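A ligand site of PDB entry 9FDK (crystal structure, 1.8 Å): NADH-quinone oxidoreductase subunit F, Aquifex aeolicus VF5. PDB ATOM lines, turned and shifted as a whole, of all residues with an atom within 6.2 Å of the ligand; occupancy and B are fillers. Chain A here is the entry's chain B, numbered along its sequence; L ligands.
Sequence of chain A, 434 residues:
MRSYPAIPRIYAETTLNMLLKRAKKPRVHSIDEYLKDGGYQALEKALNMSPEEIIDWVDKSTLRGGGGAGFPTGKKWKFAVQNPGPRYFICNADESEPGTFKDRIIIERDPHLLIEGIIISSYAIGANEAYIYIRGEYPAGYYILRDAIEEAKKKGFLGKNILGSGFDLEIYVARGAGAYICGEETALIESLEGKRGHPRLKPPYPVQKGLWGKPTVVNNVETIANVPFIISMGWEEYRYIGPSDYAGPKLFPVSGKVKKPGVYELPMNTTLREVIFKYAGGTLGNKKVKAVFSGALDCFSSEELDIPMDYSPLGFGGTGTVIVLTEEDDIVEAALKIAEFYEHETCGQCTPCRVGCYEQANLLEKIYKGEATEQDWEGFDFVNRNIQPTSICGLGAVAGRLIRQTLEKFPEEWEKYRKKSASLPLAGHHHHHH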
ATOM      1  N   ILE A 181     -33.472 -16.162  18.603  1.00  0.00           N
ATOM      2  CA  ILE A 181     -32.424 -15.213  18.938  1.00  0.00           C
ATOM      3  C   ILE A 181     -32.811 -14.398  20.166  1.00  0.00           C
ATOM      4  O   ILE A 181     -31.934 -13.873  20.831  1.00  0.00           O
ATOM      5  CB  ILE A 181     -32.073 -14.326  17.734  1.00  0.00           C
ATOM      6  CG1 ILE A 181     -30.785 -13.543  17.947  1.00  0.00           C
ATOM      7  CG2 ILE A 181     -33.225 -13.396  17.382  1.00  0.00           C
ATOM      8  CD1 ILE A 181     -29.589 -14.402  18.295  1.00  0.00           C
ATOM      9  N   HIS A 198     -32.648  -8.005  18.109  1.00  0.00           N
ATOM     10  CA  HIS A 198     -31.358  -7.849  17.469  1.00  0.00           C
ATOM     11  C   HIS A 198     -30.309  -7.781  18.564  1.00  0.00           C
ATOM     12  O   HIS A 198     -30.312  -6.845  19.364  1.00  0.00           O
ATOM     13  CB  HIS A 198     -31.321  -6.584  16.604  1.00  0.00           C
ATOM     14  CG  HIS A 198     -31.956  -6.713  15.260  1.00  0.00           C
ATOM     15  ND1 HIS A 198     -32.096  -5.603  14.444  1.00  0.00           N
ATOM     16  CD2 HIS A 198     -32.401  -7.752  14.547  1.00  0.00           C
ATOM     17  CE1 HIS A 198     -32.646  -5.964  13.290  1.00  0.00           C
ATOM     18  NE2 HIS A 198     -32.863  -7.269  13.336  1.00  0.00           N
ATOM     19  N   PRO A 199     -29.392  -8.760  18.673  1.00  0.00           N
ATOM     20  CA  PRO A 199     -28.287  -8.649  19.621  1.00  0.00           C
ATOM     21  C   PRO A 199     -27.524  -7.344  19.498  1.00  0.00           C
ATOM     22  O   PRO A 199     -27.441  -6.758  18.422  1.00  0.00           O
ATOM     23  CB  PRO A 199     -27.404  -9.862  19.313  1.00  0.00           C
ATOM     24  CG  PRO A 199     -28.394 -10.865  18.781  1.00  0.00           C
ATOM     25  CD  PRO A 199     -29.399 -10.052  17.969  1.00  0.00           C
ATOM     26  N   GLU A 345     -33.011 -18.978  12.069  1.00  0.00           N
ATOM     27  CA  GLU A 345     -32.920 -18.213  13.310  1.00  0.00           C
ATOM     28  C   GLU A 345     -31.901 -17.058  13.249  1.00  0.00           C
ATOM     29  O   GLU A 345     -31.928 -16.194  14.121  1.00  0.00           O
ATOM     30  CB  GLU A 345     -32.719 -19.162  14.491  1.00  0.00           C
ATOM     31  CG  GLU A 345     -33.874 -20.161  14.677  1.00  0.00           C
ATOM     32  CD  GLU A 345     -35.272 -19.583  14.879  1.00  0.00           C
ATOM     33  OE1 GLU A 345     -35.411 -18.380  15.247  1.00  0.00           O
ATOM     34  OE2 GLU A 345     -36.242 -20.346  14.579  1.00  0.00           O
ATOM     35  N   THR A 346     -30.984 -17.019  12.273  1.00  0.00           N
ATOM     36  CA  THR A 346     -30.083 -15.883  12.176  1.00  0.00           C
ATOM     37  C   THR A 346     -30.918 -14.604  12.081  1.00  0.00           C
ATOM     38  O   THR A 346     -31.906 -14.569  11.355  1.00  0.00           O
ATOM     39  CB  THR A 346     -29.104 -16.011  11.004  1.00  0.00           C
ATOM     40  OG1 THR A 346     -28.405 -14.769  10.953  1.00  0.00           O
ATOM     41  CG2 THR A 346     -29.785 -16.292   9.669  1.00  0.00           C
ATOM     42  N   CYS A 347     -30.541 -13.567  12.838  1.00  0.00           N
ATOM     43  CA  CYS A 347     -31.257 -12.301  12.796  1.00  0.00           C
ATOM     44  C   CYS A 347     -30.856 -11.435  11.590  1.00  0.00           C
ATOM     45  O   CYS A 347     -31.538 -10.461  11.286  1.00  0.00           O
ATOM     46  CB  CYS A 347     -31.137 -11.539  14.108  1.00  0.00           C
ATOM     47  SG  CYS A 347     -29.594 -10.604  14.326  1.00  0.00           S
ATOM     48  N   GLY A 348     -29.710 -11.748  10.954  1.00  0.00           N
ATOM     49  CA  GLY A 348     -29.321 -11.123   9.712  1.00  0.00           C
ATOM     50  C   GLY A 348     -28.491  -9.834   9.861  1.00  0.00           C
ATOM     51  O   GLY A 348     -28.151  -9.239   8.847  1.00  0.00           O
ATOM     52  N   GLN A 349     -28.149  -9.418  11.092  1.00  0.00           N
ATOM     53  CA  GLN A 349     -27.387  -8.181  11.294  1.00  0.00           C
ATOM     54  C   GLN A 349     -25.962  -8.264  10.751  1.00  0.00           C
ATOM     55  O   GLN A 349     -25.376  -7.265  10.295  1.00  0.00           O
ATOM     56  CB  GLN A 349     -27.211  -7.880  12.781  1.00  0.00           C
ATOM     57  CG  GLN A 349     -28.428  -7.280  13.468  1.00  0.00           C
ATOM     58  CD  GLN A 349     -28.080  -6.845  14.880  1.00  0.00           C
ATOM     59  OE1 GLN A 349     -27.970  -7.641  15.827  1.00  0.00           O
ATOM     60  NE2 GLN A 349     -27.851  -5.554  15.012  1.00  0.00           N
ATOM     61  N   CYS A 350     -25.356  -9.451  10.874  1.00  0.00           N
ATOM     62  CA  CYS A 350     -23.968  -9.672  10.507  1.00  0.00           C
ATOM     63  C   CYS A 350     -23.952 -10.420   9.174  1.00  0.00           C
ATOM     64  O   CYS A 350     -24.667 -11.402   9.007  1.00  0.00           O
ATOM     65  CB  CYS A 350     -23.201 -10.433  11.575  1.00  0.00           C
ATOM     66  SG  CYS A 350     -23.551  -9.937  13.287  1.00  0.00           S
ATOM     67  N   THR A 351     -23.107  -9.958   8.249  1.00  0.00           N
ATOM     68  CA  THR A 351     -23.190 -10.453   6.878  1.00  0.00           C
ATOM     69  C   THR A 351     -22.803 -11.946   6.820  1.00  0.00           C
ATOM     70  O   THR A 351     -23.532 -12.747   6.261  1.00  0.00           O
ATOM     71  CB  THR A 351     -22.374  -9.549   5.947  1.00  0.00           C
ATOM     72  OG1 THR A 351     -23.216  -8.407   5.812  1.00  0.00           O
ATOM     73  CG2 THR A 351     -22.115 -10.193   4.601  1.00  0.00           C
ATOM     74  N   CYS A 353     -22.879 -14.346   8.993  1.00  0.00           N
ATOM     75  CA  CYS A 353     -23.929 -15.107   9.638  1.00  0.00           C
ATOM     76  C   CYS A 353     -25.205 -15.159   8.783  1.00  0.00           C
ATOM     77  O   CYS A 353     -25.752 -16.237   8.549  1.00  0.00           O
ATOM     78  CB  CYS A 353     -24.280 -14.500  10.987  1.00  0.00           C
ATOM     79  SG  CYS A 353     -25.495 -15.434  11.954  1.00  0.00           S
ATOM     80  N   ARG A 354     -25.643 -13.989   8.311  1.00  0.00           N
ATOM     81  CA  ARG A 354     -26.829 -13.891   7.476  1.00  0.00           C
ATOM     82  C   ARG A 354     -26.707 -14.788   6.240  1.00  0.00           C
ATOM     83  O   ARG A 354     -27.585 -15.613   5.957  1.00  0.00           O
ATOM     84  CB  ARG A 354     -27.056 -12.438   7.037  1.00  0.00           C
ATOM     85  CG  ARG A 354     -28.267 -12.200   6.147  1.00  0.00           C
ATOM     86  CD  ARG A 354     -28.474 -10.721   5.789  1.00  0.00           C
ATOM     87  NE  ARG A 354     -27.416 -10.161   4.968  1.00  0.00           N
ATOM     88  CZ  ARG A 354     -26.429  -9.370   5.386  1.00  0.00           C
ATOM     89  NH1 ARG A 354     -26.367  -8.992   6.675  1.00  0.00           N
ATOM     90  NH2 ARG A 354     -25.525  -8.945   4.490  1.00  0.00           N
ATOM     91  N   CYS A 357     -25.546 -18.805   7.253  1.00  0.00           N
ATOM     92  CA  CYS A 357     -26.561 -19.718   7.758  1.00  0.00           C
ATOM     93  C   CYS A 357     -27.494 -20.137   6.608  1.00  0.00           C
ATOM     94  O   CYS A 357     -27.901 -21.304   6.553  1.00  0.00           O
ATOM     95  CB  CYS A 357     -27.364 -19.147   8.914  1.00  0.00           C
ATOM     96  SG  CYS A 357     -26.400 -18.929  10.428  1.00  0.00           S
ATOM     97  N   ILE A 387     -18.983 -18.694   8.844  1.00  0.00           N
ATOM     98  CA  ILE A 387     -20.191 -18.070   9.355  1.00  0.00           C
ATOM     99  C   ILE A 387     -19.831 -17.081  10.465  1.00  0.00           C
ATOM    100  O   ILE A 387     -20.489 -16.053  10.621  1.00  0.00           O
ATOM    101  CB  ILE A 387     -21.197 -19.127   9.836  1.00  0.00           C
ATOM    102  CG1 ILE A 387     -21.474 -20.177   8.740  1.00  0.00           C
ATOM    103  CG2 ILE A 387     -22.484 -18.487  10.335  1.00  0.00           C
ATOM    104  CD1 ILE A 387     -22.419 -21.286   9.170  1.00  0.00           C
ATOM    105  N   THR A 390     -16.892 -11.597  12.093  1.00  0.00           N
ATOM    106  CA  THR A 390     -17.593 -10.342  12.353  1.00  0.00           C
ATOM    107  C   THR A 390     -18.853 -10.529  13.205  1.00  0.00           C
ATOM    108  O   THR A 390     -19.479  -9.527  13.543  1.00  0.00           O
ATOM    109  CB  THR A 390     -17.891  -9.557  11.069  1.00  0.00           C
ATOM    110  OG1 THR A 390     -19.092 -10.022  10.447  1.00  0.00           O
ATOM    111  CG2 THR A 390     -16.727  -9.577  10.091  1.00  0.00           C
ATOM    112  N   SER A 391     -19.224 -11.774  13.582  1.00  0.00           N
ATOM    113  CA  SER A 391     -20.432 -12.028  14.348  1.00  0.00           C
ATOM    114  C   SER A 391     -20.379 -11.294  15.690  1.00  0.00           C
ATOM    115  O   SER A 391     -19.336 -11.215  16.330  1.00  0.00           O
ATOM    116  CB  SER A 391     -20.651 -13.508  14.578  1.00  0.00           C
ATOM    117  OG  SER A 391     -19.519 -14.077  15.211  1.00  0.00           O
ATOM    118  N   ILE A 392     -21.520 -10.760  16.120  1.00  0.00           N
ATOM    119  CA  ILE A 392     -21.562 -10.047  17.388  1.00  0.00           C
ATOM    120  C   ILE A 392     -22.320 -10.846  18.446  1.00  0.00           C
ATOM    121  O   ILE A 392     -22.544 -10.326  19.536  1.00  0.00           O
ATOM    122  CB  ILE A 392     -22.114  -8.625  17.207  1.00  0.00           C
ATOM    123  CG1 ILE A 392     -23.590  -8.589  16.799  1.00  0.00           C
ATOM    124  CG2 ILE A 392     -21.255  -7.811  16.235  1.00  0.00           C
ATOM    125  CD1 ILE A 392     -24.132  -7.178  16.618  1.00  0.00           C
ATOM    126  N   CYS A 393     -22.768 -12.074  18.137  1.00  0.00           N
ATOM    127  CA  CYS A 393     -23.388 -12.912  19.147  1.00  0.00           C
ATOM    128  C   CYS A 393     -22.986 -14.369  18.933  1.00  0.00           C
ATOM    129  O   CYS A 393     -22.390 -14.706  17.926  1.00  0.00           O
ATOM    130  CB  CYS A 393     -24.895 -12.712  19.224  1.00  0.00           C
ATOM    131  SG  CYS A 393     -25.910 -13.860  18.254  1.00  0.00           S
ATOM    132  N   GLY A 394     -23.316 -15.211  19.904  1.00  0.00           N
ATOM    133  CA  GLY A 394     -22.895 -16.604  19.913  1.00  0.00           C
ATOM    134  C   GLY A 394     -23.459 -17.436  18.754  1.00  0.00           C
ATOM    135  O   GLY A 394     -22.874 -18.447  18.408  1.00  0.00           O
ATOM    136  N   LEU A 395     -24.601 -17.040  18.170  1.00  0.00           N
ATOM    137  CA  LEU A 395     -25.227 -17.819  17.122  1.00  0.00           C
ATOM    138  C   LEU A 395     -24.272 -17.957  15.923  1.00  0.00           C
ATOM    139  O   LEU A 395     -24.032 -19.069  15.452  1.00  0.00           O
ATOM    140  CB  LEU A 395     -26.575 -17.240  16.696  1.00  0.00           C
ATOM    141  CG  LEU A 395     -27.430 -18.117  15.779  1.00  0.00           C
ATOM    142  CD1 LEU A 395     -28.897 -17.831  15.931  1.00  0.00           C
ATOM    143  CD2 LEU A 395     -27.025 -17.980  14.307  1.00  0.00           C
ATOM    144  N   GLY A 396     -23.778 -16.830  15.413  1.00  0.00           N
ATOM    145  CA  GLY A 396     -22.845 -16.864  14.296  1.00  0.00           C
ATOM    146  C   GLY A 396     -21.575 -17.642  14.645  1.00  0.00           C
ATOM    147  O   GLY A 396     -21.010 -18.326  13.801  1.00  0.00           O
ATOM    148  N   ALA A 397     -21.159 -17.562  15.920  1.00  0.00           N
ATOM    149  CA  ALA A 397     -19.969 -18.250  16.393  1.00  0.00           C
ATOM    150  C   ALA A 397     -20.114 -19.777  16.350  1.00  0.00           C
ATOM    151  O   ALA A 397     -19.115 -20.476  16.208  1.00  0.00           O
ATOM    152  CB  ALA A 397     -19.663 -17.787  17.815  1.00  0.00           C
HETATM  153 FE1  LIG L   1     -27.715 -11.878  14.359  1.00  0.00          FE
HETATM  154 FE2  LIG L   1     -25.990 -13.917  13.560  1.00  0.00          FE
HETATM  155 FE3  LIG L   1     -25.954 -13.035  16.132  1.00  0.00          FE
HETATM  156 FE4  LIG L   1     -25.040 -11.437  14.092  1.00  0.00          FE
HETATM  157  S1  LIG L   1     -24.131 -13.462  14.821  1.00  0.00           S
HETATM  158  S2  LIG L   1     -26.316 -10.771  15.816  1.00  0.00           S
HETATM  159  S3  LIG L   1     -26.531 -12.022  12.407  1.00  0.00           S
HETATM  160  S4  LIG L   1     -27.726 -14.052  15.065  1.00  0.00           S
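The backbone NH (N) of Cys 347 sits close to a sulfur (S4) of the ligand (3.6 Å).
An iron atom (FE1) of the ligand is bound by the side-chain sulfur (SG) of Cys 347 (2.3 Å).
S1 of the ligand lies close to N of Gly 396 (3.4 Å).
SG of Cys 393 is bound to FE3 of the ligand (2.3 Å).
The backbone NH (N) of Cys 350 sits close to a sulfur (S3) of the ligand (3.2 Å).
The backbone NH (N) of Gln 349 lies close to a sulfur (S3) of the ligand (3.3 Å).
The backbone NH (N) of Gly 348 sits close to a sulfur (S3) of the ligand, at 3.5 Å.
The side-chain sulfur (SG) of Cys 350 is bound to an iron atom (FE4) of the ligand (2.3 Å).
SG of Cys 353 is bound to FE2 of the ligand (2.3 Å).
The side-chain amide oxygen (OE1) of Gln 349 sits close to a sulfur (S2) of the ligand (3.5 Å).
S3 of the ligand sits close to OG1 of Thr 346 (3.6 Å).
O of Cys 353 is in hydrogen-bond range of SG of Cys 357 (3.3 Å).
The backbone NH (N) of Gly 348 lies within hydrogen-bond range of the side-chain hydroxyl (OG1) of Thr 346 (3.3 Å).
OE1 of Gln 349 lies close to SG of Cys 347.
The side-chain amide oxygen (OE1) of Gln 349 sits close to the backbone carbonyl oxygen (O) of Pro 199, 2.8 Å away.
The backbone carbonyl oxygen of Ile 387 lies within hydrogen-bond range of the backbone NH of Cys 353 (3.4 Å).
SG of Cys 393 lies close to N of Leu 395, 3.4 Å away.
The side-chain sulfur (SG) of Cys 350 lies close to the backbone NH (N) of Ile 392 (3.6 Å).
NH1 of Arg 354 lies within hydrogen-bond range of O of Gly 348, 2.8 Å away.
Ile 181 touches the ligand (CD1 to S4, 3.7 Å).
Pro 199 touches the ligand.
CB of Ser 391 touches S1 of the ligand, 3.5 Å away.
Ile 392 touches the ligand (CG1 to S2, 3.6 Å).
Leu 395 touches the ligand (CB to S4, 3.8 Å).
Of the 22 residues printed, 13 come within 4 Å of the ligand.
The nearest printed residue that does not touch the ligand is Arg 354 (4.6 Å).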
